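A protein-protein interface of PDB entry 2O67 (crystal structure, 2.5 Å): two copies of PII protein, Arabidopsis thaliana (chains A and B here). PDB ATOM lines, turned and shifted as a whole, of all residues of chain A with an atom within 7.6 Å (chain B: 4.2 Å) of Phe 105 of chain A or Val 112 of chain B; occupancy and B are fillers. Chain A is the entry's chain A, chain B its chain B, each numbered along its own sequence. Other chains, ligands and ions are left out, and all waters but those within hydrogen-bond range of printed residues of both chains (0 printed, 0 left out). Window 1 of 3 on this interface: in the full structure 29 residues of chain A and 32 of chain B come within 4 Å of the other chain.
The backbone carbonyl oxygen of Phe 13 of chain B lies within hydrogen-bond range of the backbone NH of Val 109 of chain B, at 2.9 Å.
N of Ile 19 of chain A is in hydrogen-bond range of O of Lys 103 of chain A (2.8 Å).
O of Val 112 of chain B lies within hydrogen-bond range of N of Gly 121 of chain B, 3.1 Å away.
The backbone NH (N) of Lys 15 of chain A sits at hydrogen-bond distance from the backbone carbonyl oxygen (O) of Leu 107 of chain A (2.6 Å).
OD2 of Asp 111 of chain B is in salt-bridge range of NE of Arg 120 of chain B, 2.7 Å away.
The backbone carbonyl oxygen of Glu 17 of chain A sits at hydrogen-bond distance from the backbone NH of Phe 105 of chain A, 2.7 Å away.
Phe 105 of chain A touches just these residues of chain B: Val 77, Asp 111 and Val 112.
Of chain A, only Lys 103 (3.8 Å), Ile 104 (3.4 Å) and Phe 105 (3.9 Å) come within 4 Å of Val 112 of chain B.
Of the printed residues of chain A, Ile 113 of chain B touches Ile 87 (3.9 Å), Lys 103 (3.3 Å), Ile 104 (2.8 Å) and Val 106 (3.997 Å).
Of the printed residues of chain B, Lys 103 of chain A touches Val 112 (3.8 Å), Ile 113 (3.3 Å) and Ala 124 (2.8 Å).
Of the printed residues of chain B, Ile 87 of chain A touches Ile 113 and Arg 120.
Printed residues of chain A within 4 Å of Asp 111 of chain B: Ile 104, Phe 105 and Val 106.
Of the printed residues of chain B, Leu 107 of chain A touches Val 109 (3.95 Å).
Gly 102 of chain A touches none of the printed residues of chain B.
The nearest printed residue of chain B that does not touch Phe 105 of chain A is Val 109 of chain B (4.3 Å).
The nearest residue of chain A that does not touch Val 112 of chain B is Val 106 of chain A (5.1 Å).
The nearest printed residue of chain A that does not touch Arg 120 of chain B is Val 83 of chain A (5.7 Å).
The backbone NH (N) of Ile 104 of chain A is in hydrogen-bond range of the backbone carbonyl oxygen (O) of Ile 113 of chain B, at 2.8 Å.
The side-chain amino group of Lys 103 of chain A is in hydrogen-bond range of the backbone carbonyl oxygen of Ala 124 of chain B, at 2.8 Å.
N of Val 106 of chain A sits at hydrogen-bond distance from O of Asp 111 of chain B (2.9 Å).
Among the printed residues, merely in contact across the chains: Ile 87 of chain A with Ile 113 of chain B (3.9 Å), Ile 87 of chain A with Arg 120 of chain B (3.8 Å), Lys 103 of chain A with Val 112 of chain B (3.8 Å), Lys 103 of chain A with Ile 113 of chain B (3.3 Å), Ile 104 of chain A with Asp 111 of chain B (3.9 Å), Ile 104 of chain A with Val 112 of chain B (3.4 Å), Phe 105 of chain A with Val 77 of chain B (3.6 Å), Phe 105 of chain A with Asp 111 of chain B (3.5 Å), Phe 105 of chain A with Val 112 of chain B (3.9 Å), Val 106 of chain A with Val 109 of chain B (3.4 Å), Val 106 of chain A with Ile 113 of chain B (3.997 Å) and Leu 107 of chain A with Val 109 of chain B (3.95 Å).
Hydrophobic or aromatic side chains of chain B within 4 Å of the printed part of chain A: Val 77, Val 109, Val 112 and Ile 113.
Along chain B the printed residues that touch a printed residue of chain A span positions 77 to 124.
Of the 18 printed residues of chain A, 6 touch a printed residue of chain B.
Hydrophobic or aromatic side chains of chain A that line the printed part of chain B: Ile 87, Ile 104, Phe 105, Val 106 and Leu 107.
Among the printed residues, 15 pairs touch across the chains.
No position is printed for both chains.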
ATOM      1  N   TYR A  14     -11.893  -1.559   2.471  1.00  0.00           N
ATOM      2  CA  TYR A  14     -12.388  -0.190   2.491  1.00  0.00           C
ATOM      3  C   TYR A  14     -11.844   0.506   3.714  1.00  0.00           C
ATOM      4  O   TYR A  14     -11.741  -0.105   4.779  1.00  0.00           O
ATOM      5  CB  TYR A  14     -13.920  -0.148   2.525  1.00  0.00           C
ATOM      6  CG  TYR A  14     -14.584  -0.520   1.225  1.00  0.00           C
ATOM      7  CD1 TYR A  14     -14.817  -1.859   0.905  1.00  0.00           C
ATOM      8  CD2 TYR A  14     -14.994   0.459   0.318  1.00  0.00           C
ATOM      9  CE1 TYR A  14     -15.422  -2.220  -0.293  1.00  0.00           C
ATOM     10  CE2 TYR A  14     -15.608   0.105  -0.894  1.00  0.00           C
ATOM     11  CZ  TYR A  14     -15.815  -1.244  -1.183  1.00  0.00           C
ATOM     12  OH  TYR A  14     -16.417  -1.640  -2.360  1.00  0.00           O
ATOM     13  N   LYS A  15     -11.485   1.777   3.560  1.00  0.00           N
ATOM     14  CA  LYS A  15     -11.157   2.608   4.705  1.00  0.00           C
ATOM     15  C   LYS A  15     -12.418   3.278   5.236  1.00  0.00           C
ATOM     16  O   LYS A  15     -13.212   3.834   4.472  1.00  0.00           O
ATOM     17  CB  LYS A  15     -10.128   3.680   4.357  1.00  0.00           C
ATOM     18  CG  LYS A  15      -9.541   4.305   5.615  1.00  0.00           C
ATOM     19  CD  LYS A  15      -9.066   5.702   5.395  1.00  0.00           C
ATOM     20  CE  LYS A  15      -7.561   5.761   5.326  1.00  0.00           C
ATOM     21  NZ  LYS A  15      -7.165   7.187   5.196  1.00  0.00           N
ATOM     22  N   VAL A  16     -12.596   3.211   6.548  1.00  0.00           N
ATOM     23  CA  VAL A  16     -13.670   3.943   7.207  1.00  0.00           C
ATOM     24  C   VAL A  16     -13.046   5.081   8.011  1.00  0.00           C
ATOM     25  O   VAL A  16     -12.195   4.866   8.880  1.00  0.00           O
ATOM     26  CB  VAL A  16     -14.557   3.032   8.091  1.00  0.00           C
ATOM     27  CG1 VAL A  16     -15.758   3.798   8.608  1.00  0.00           C
ATOM     28  CG2 VAL A  16     -15.036   1.835   7.296  1.00  0.00           C
ATOM     29  N   GLU A  17     -13.471   6.293   7.681  1.00  0.00           N
ATOM     30  CA  GLU A  17     -12.923   7.512   8.249  1.00  0.00           C
ATOM     31  C   GLU A  17     -14.041   8.188   9.022  1.00  0.00           C
ATOM     32  O   GLU A  17     -15.062   8.550   8.440  1.00  0.00           O
ATOM     33  CB  GLU A  17     -12.490   8.423   7.103  1.00  0.00           C
ATOM     34  CG  GLU A  17     -11.185   9.139   7.285  1.00  0.00           C
ATOM     35  CD  GLU A  17     -10.688   9.724   5.970  1.00  0.00           C
ATOM     36  OE1 GLU A  17     -11.407  10.566   5.385  1.00  0.00           O
ATOM     37  OE2 GLU A  17      -9.587   9.339   5.517  1.00  0.00           O
ATOM     38  N   ALA A  18     -13.861   8.354  10.326  1.00  0.00           N
ATOM     39  CA  ALA A  18     -14.875   9.019  11.144  1.00  0.00           C
ATOM     40  C   ALA A  18     -14.360  10.325  11.736  1.00  0.00           C
ATOM     41  O   ALA A  18     -13.386  10.323  12.493  1.00  0.00           O
ATOM     42  CB  ALA A  18     -15.359   8.091  12.256  1.00  0.00           C
ATOM     43  N   ILE A  19     -15.011  11.434  11.389  1.00  0.00           N
ATOM     44  CA  ILE A  19     -14.692  12.722  11.997  1.00  0.00           C
ATOM     45  C   ILE A  19     -15.688  12.965  13.122  1.00  0.00           C
ATOM     46  O   ILE A  19     -16.847  13.302  12.874  1.00  0.00           O
ATOM     47  CB  ILE A  19     -14.723  13.901  10.983  1.00  0.00           C
ATOM     48  CG1 ILE A  19     -14.163  13.485   9.612  1.00  0.00           C
ATOM     49  CG2 ILE A  19     -13.996  15.127  11.562  1.00  0.00           C
ATOM     50  CD1 ILE A  19     -12.688  13.167   9.592  1.00  0.00           C
ATOM     51  N   LYS A  73     -10.142  12.654  13.707  1.00  0.00           N
ATOM     52  CA  LYS A  73     -10.351  11.738  12.605  1.00  0.00           C
ATOM     53  C   LYS A  73      -9.972  10.347  13.093  1.00  0.00           C
ATOM     54  O   LYS A  73      -8.874  10.141  13.602  1.00  0.00           O
ATOM     55  CB  LYS A  73      -9.507  12.162  11.395  1.00  0.00           C
ATOM     56  CG  LYS A  73      -9.710  11.329  10.124  1.00  0.00           C
ATOM     57  CD  LYS A  73      -9.304  12.100   8.866  1.00  0.00           C
ATOM     58  CE  LYS A  73      -7.797  12.145   8.689  1.00  0.00           C
ATOM     59  NZ  LYS A  73      -7.380  13.149   7.671  1.00  0.00           N
ATOM     60  N   MET A  74     -10.892   9.399  12.961  1.00  0.00           N
ATOM     61  CA  MET A  74     -10.627   8.025  13.360  1.00  0.00           C
ATOM     62  C   MET A  74     -10.612   7.137  12.130  1.00  0.00           C
ATOM     63  O   MET A  74     -11.574   7.117  11.357  1.00  0.00           O
ATOM     64  CB  MET A  74     -11.664   7.541  14.365  1.00  0.00           C
ATOM     65  CG  MET A  74     -11.757   8.407  15.610  1.00  0.00           C
ATOM     66  SD  MET A  74     -12.768   7.674  16.906  1.00  0.00           S
ATOM     67  CE  MET A  74     -11.658   6.409  17.528  1.00  0.00           C
ATOM     68  N   ILE A  76      -9.834   3.357  10.243  1.00  0.00           N
ATOM     69  CA  ILE A  76      -9.683   1.911  10.293  1.00  0.00           C
ATOM     70  C   ILE A  76      -9.897   1.337   8.894  1.00  0.00           C
ATOM     71  O   ILE A  76     -10.753   1.814   8.148  1.00  0.00           O
ATOM     72  CB  ILE A  76     -10.634   1.269  11.364  1.00  0.00           C
ATOM     73  CG1 ILE A  76     -10.370  -0.231  11.528  1.00  0.00           C
ATOM     74  CG2 ILE A  76     -12.116   1.543  11.059  1.00  0.00           C
ATOM     75  CD1 ILE A  76      -9.088  -0.552  12.235  1.00  0.00           C
ATOM     76  N   VAL A  83     -17.780  -3.655   6.873  1.00  0.00           N
ATOM     77  CA  VAL A  83     -18.039  -2.218   6.746  1.00  0.00           C
ATOM     78  C   VAL A  83     -19.293  -1.770   7.503  1.00  0.00           C
ATOM     79  O   VAL A  83     -19.252  -0.792   8.252  1.00  0.00           O
ATOM     80  CB  VAL A  83     -18.105  -1.781   5.252  1.00  0.00           C
ATOM     81  CG1 VAL A  83     -18.548  -0.337   5.120  1.00  0.00           C
ATOM     82  CG2 VAL A  83     -16.747  -1.990   4.563  1.00  0.00           C
ATOM     83  N   ILE A  87     -19.432   0.833  10.619  1.00  0.00           N
ATOM     84  CA  ILE A  87     -20.220   2.064  10.537  1.00  0.00           C
ATOM     85  C   ILE A  87     -21.157   2.195  11.741  1.00  0.00           C
ATOM     86  O   ILE A  87     -21.130   3.204  12.444  1.00  0.00           O
ATOM     87  CB  ILE A  87     -21.040   2.150   9.220  1.00  0.00           C
ATOM     88  CG1 ILE A  87     -20.116   2.300   8.011  1.00  0.00           C
ATOM     89  CG2 ILE A  87     -22.056   3.306   9.279  1.00  0.00           C
ATOM     90  CD1 ILE A  87     -20.827   2.154   6.675  1.00  0.00           C
ATOM     91  N   ILE A  90     -19.411   2.743  15.129  1.00  0.00           N
ATOM     92  CA  ILE A  90     -18.866   4.096  15.287  1.00  0.00           C
ATOM     93  C   ILE A  90     -19.991   5.063  15.654  1.00  0.00           C
ATOM     94  O   ILE A  90     -19.822   5.884  16.552  1.00  0.00           O
ATOM     95  CB  ILE A  90     -18.088   4.578  14.031  1.00  0.00           C
ATOM     96  CG1 ILE A  90     -16.808   3.754  13.853  1.00  0.00           C
ATOM     97  CG2 ILE A  90     -17.738   6.063  14.139  1.00  0.00           C
ATOM     98  CD1 ILE A  90     -16.268   3.765  12.439  1.00  0.00           C
ATOM     99  N   GLY A 102     -20.516  14.627  13.847  1.00  0.00           N
ATOM    100  CA  GLY A 102     -19.533  14.336  12.815  1.00  0.00           C
ATOM    101  C   GLY A 102     -20.059  13.567  11.616  1.00  0.00           C
ATOM    102  O   GLY A 102     -21.276  13.449  11.413  1.00  0.00           O
ATOM    103  N   LYS A 103     -19.127  13.052  10.817  1.00  0.00           N
ATOM    104  CA  LYS A 103     -19.453  12.275   9.624  1.00  0.00           C
ATOM    105  C   LYS A 103     -18.581  11.038   9.522  1.00  0.00           C
ATOM    106  O   LYS A 103     -17.506  10.970  10.125  1.00  0.00           O
ATOM    107  CB  LYS A 103     -19.282  13.113   8.353  1.00  0.00           C
ATOM    108  CG  LYS A 103     -20.335  14.199   8.162  1.00  0.00           C
ATOM    109  CD  LYS A 103     -20.584  14.466   6.683  1.00  0.00           C
ATOM    110  CE  LYS A 103     -21.043  15.889   6.439  1.00  0.00           C
ATOM    111  NZ  LYS A 103     -22.426  16.127   6.903  1.00  0.00           N
ATOM    112  N   ILE A 104     -19.052  10.064   8.751  1.00  0.00           N
ATOM    113  CA  ILE A 104     -18.275   8.868   8.438  1.00  0.00           C
ATOM    114  C   ILE A 104     -18.131   8.797   6.929  1.00  0.00           C
ATOM    115  O   ILE A 104     -19.115   8.943   6.202  1.00  0.00           O
ATOM    116  CB  ILE A 104     -18.944   7.565   8.963  1.00  0.00           C
ATOM    117  CG1 ILE A 104     -19.012   7.568  10.493  1.00  0.00           C
ATOM    118  CG2 ILE A 104     -18.185   6.335   8.468  1.00  0.00           C
ATOM    119  CD1 ILE A 104     -20.057   6.641  11.060  1.00  0.00           C
ATOM    120  N   PHE A 105     -16.904   8.594   6.465  1.00  0.00           N
ATOM    121  CA  PHE A 105     -16.642   8.416   5.041  1.00  0.00           C
ATOM    122  C   PHE A 105     -16.125   7.004   4.808  1.00  0.00           C
ATOM    123  O   PHE A 105     -15.315   6.486   5.589  1.00  0.00           O
ATOM    124  CB  PHE A 105     -15.629   9.455   4.535  1.00  0.00           C
ATOM    125  CG  PHE A 105     -15.975  10.882   4.895  1.00  0.00           C
ATOM    126  CD1 PHE A 105     -17.031  11.540   4.272  1.00  0.00           C
ATOM    127  CD2 PHE A 105     -15.234  11.571   5.854  1.00  0.00           C
ATOM    128  CE1 PHE A 105     -17.349  12.875   4.604  1.00  0.00           C
ATOM    129  CE2 PHE A 105     -15.538  12.903   6.190  1.00  0.00           C
ATOM    130  CZ  PHE A 105     -16.601  13.553   5.557  1.00  0.00           C
ATOM    131  N   VAL A 106     -16.611   6.383   3.741  1.00  0.00           N
ATOM    132  CA  VAL A 106     -16.177   5.050   3.348  1.00  0.00           C
ATOM    133  C   VAL A 106     -15.442   5.155   2.012  1.00  0.00           C
ATOM    134  O   VAL A 106     -16.025   5.586   1.006  1.00  0.00           O
ATOM    135  CB  VAL A 106     -17.379   4.071   3.232  1.00  0.00           C
ATOM    136  CG1 VAL A 106     -16.927   2.696   2.729  1.00  0.00           C
ATOM    137  CG2 VAL A 106     -18.105   3.949   4.576  1.00  0.00           C
ATOM    138  N   LEU A 107     -14.171   4.756   2.014  1.00  0.00           N
ATOM    139  CA  LEU A 107     -13.295   4.871   0.840  1.00  0.00           C
ATOM    140  C   LEU A 107     -12.731   3.510   0.445  1.00  0.00           C
ATOM    141  O   LEU A 107     -12.333   2.744   1.321  1.00  0.00           O
ATOM    142  CB  LEU A 107     -12.119   5.824   1.125  1.00  0.00           C
ATOM    143  CG  LEU A 107     -12.393   7.291   1.460  1.00  0.00           C
ATOM    144  CD1 LEU A 107     -12.479   7.487   2.966  1.00  0.00           C
ATOM    145  CD2 LEU A 107     -11.316   8.190   0.861  1.00  0.00           C
ATOM    146  N   PHE B  13     -19.514   9.987  -4.793  1.00  0.00           N
ATOM    147  CA  PHE B  13     -18.805  10.983  -3.999  1.00  0.00           C
ATOM    148  C   PHE B  13     -17.302  10.921  -4.237  1.00  0.00           C
ATOM    149  O   PHE B  13     -16.766   9.872  -4.611  1.00  0.00           O
ATOM    150  CB  PHE B  13     -19.095  10.786  -2.507  1.00  0.00           C
ATOM    151  CG  PHE B  13     -20.538  10.976  -2.141  1.00  0.00           C
ATOM    152  CD1 PHE B  13     -21.061  12.259  -1.967  1.00  0.00           C
ATOM    153  CD2 PHE B  13     -21.378   9.877  -1.984  1.00  0.00           C
ATOM    154  CE1 PHE B  13     -22.404  12.446  -1.638  1.00  0.00           C
ATOM    155  CE2 PHE B  13     -22.723  10.049  -1.657  1.00  0.00           C
ATOM    156  CZ  PHE B  13     -23.236  11.337  -1.482  1.00  0.00           C
ATOM    157  N   VAL B  77     -15.466  16.365   1.140  1.00  0.00           N
ATOM    158  CA  VAL B  77     -16.141  15.321   0.382  1.00  0.00           C
ATOM    159  C   VAL B  77     -17.381  15.920  -0.267  1.00  0.00           C
ATOM    160  O   VAL B  77     -18.187  16.574   0.392  1.00  0.00           O
ATOM    161  CB  VAL B  77     -16.469  14.107   1.272  1.00  0.00           C
ATOM    162  CG1 VAL B  77     -17.346  13.115   0.537  1.00  0.00           C
ATOM    163  CG2 VAL B  77     -15.178  13.436   1.732  1.00  0.00           C
ATOM    164  N   VAL B 109     -15.108   8.329  -2.863  1.00  0.00           N
ATOM    165  CA  VAL B 109     -15.748   7.989  -1.587  1.00  0.00           C
ATOM    166  C   VAL B 109     -17.011   7.161  -1.852  1.00  0.00           C
ATOM    167  O   VAL B 109     -17.926   7.616  -2.550  1.00  0.00           O
ATOM    168  CB  VAL B 109     -16.060   9.254  -0.748  1.00  0.00           C
ATOM    169  CG1 VAL B 109     -16.941   8.917   0.461  1.00  0.00           C
ATOM    170  CG2 VAL B 109     -14.764   9.921  -0.293  1.00  0.00           C
ATOM    171  N   ASP B 111     -19.332   5.980   0.291  1.00  0.00           N
ATOM    172  CA  ASP B 111     -20.505   6.397   1.036  1.00  0.00           C
ATOM    173  C   ASP B 111     -20.174   7.450   2.092  1.00  0.00           C
ATOM    174  O   ASP B 111     -19.057   7.498   2.614  1.00  0.00           O
ATOM    175  CB  ASP B 111     -21.184   5.182   1.690  1.00  0.00           C
ATOM    176  CG  ASP B 111     -22.682   5.379   1.883  1.00  0.00           C
ATOM    177  OD1 ASP B 111     -23.247   6.377   1.365  1.00  0.00           O
ATOM    178  OD2 ASP B 111     -23.299   4.527   2.552  1.00  0.00           O
ATOM    179  N   VAL B 112     -21.170   8.286   2.391  1.00  0.00           N
ATOM    180  CA  VAL B 112     -21.093   9.304   3.438  1.00  0.00           C
ATOM    181  C   VAL B 112     -22.257   9.097   4.410  1.00  0.00           C
ATOM    182  O   VAL B 112     -23.410   8.965   3.988  1.00  0.00           O
ATOM    183  CB  VAL B 112     -21.199  10.732   2.856  1.00  0.00           C
ATOM    184  CG1 VAL B 112     -21.018  11.784   3.960  1.00  0.00           C
ATOM    185  CG2 VAL B 112     -20.178  10.935   1.754  1.00  0.00           C
ATOM    186  N   ILE B 113     -21.943   9.080   5.703  1.00  0.00           N
ATOM    187  CA  ILE B 113     -22.932   8.886   6.757  1.00  0.00           C
ATOM    188  C   ILE B 113     -22.872  10.035   7.772  1.00  0.00           C
ATOM    189  O   ILE B 113     -21.795  10.386   8.254  1.00  0.00           O
ATOM    190  CB  ILE B 113     -22.728   7.521   7.505  1.00  0.00           C
ATOM    191  CG1 ILE B 113     -22.606   6.333   6.534  1.00  0.00           C
ATOM    192  CG2 ILE B 113     -23.864   7.260   8.488  1.00  0.00           C
ATOM    193  CD1 ILE B 113     -21.187   6.030   6.040  1.00  0.00           C
ATOM    194  N   GLU B 119     -28.168   9.152   8.529  1.00  0.00           N
ATOM    195  CA  GLU B 119     -28.460   9.436   7.126  1.00  0.00           C
ATOM    196  C   GLU B 119     -27.261   9.126   6.242  1.00  0.00           C
ATOM    197  O   GLU B 119     -26.118   9.390   6.621  1.00  0.00           O
ATOM    198  CB  GLU B 119     -28.843  10.908   6.952  1.00  0.00           C
ATOM    199  CG  GLU B 119     -30.234  11.274   7.460  1.00  0.00           C
ATOM    200  CD  GLU B 119     -30.438  12.775   7.557  1.00  0.00           C
ATOM    201  OE1 GLU B 119     -29.692  13.436   8.319  1.00  0.00           O
ATOM    202  OE2 GLU B 119     -31.351  13.293   6.874  1.00  0.00           O
ATOM    203  N   ARG B 120     -27.538   8.571   5.062  1.00  0.00           N
ATOM    204  CA  ARG B 120     -26.500   8.147   4.121  1.00  0.00           C
ATOM    205  C   ARG B 120     -26.778   8.692   2.731  1.00  0.00           C
ATOM    206  O   ARG B 120     -27.931   8.897   2.360  1.00  0.00           O
ATOM    207  CB  ARG B 120     -26.410   6.619   4.059  1.00  0.00           C
ATOM    208  CG  ARG B 120     -25.909   5.985   5.325  1.00  0.00           C
ATOM    209  CD  ARG B 120     -26.076   4.479   5.325  1.00  0.00           C
ATOM    210  NE  ARG B 120     -25.056   3.791   4.534  1.00  0.00           N
ATOM    211  CZ  ARG B 120     -24.539   2.602   4.848  1.00  0.00           C
ATOM    212  NH1 ARG B 120     -24.926   1.969   5.950  1.00  0.00           N
ATOM    213  NH2 ARG B 120     -23.625   2.048   4.065  1.00  0.00           N
ATOM    214  N   GLY B 121     -25.714   8.917   1.964  1.00  0.00           N
ATOM    215  CA  GLY B 121     -25.842   9.376   0.588  1.00  0.00           C
ATOM    216  C   GLY B 121     -25.979  10.879   0.534  1.00  0.00           C
ATOM    217  O   GLY B 121     -25.327  11.584   1.306  1.00  0.00           O
ATOM    218  N   ALA B 124     -26.750  13.514   3.474  1.00  0.00           N
ATOM    219  CA  ALA B 124     -25.695  13.375   4.479  1.00  0.00           C
ATOM    220  C   ALA B 124     -24.421  14.145   4.122  1.00  0.00           C
ATOM    221  O   ALA B 124     -23.586  14.402   4.995  1.00  0.00           O
ATOM    222  CB  ALA B 124     -25.373  11.903   4.696  1.00  0.00           C
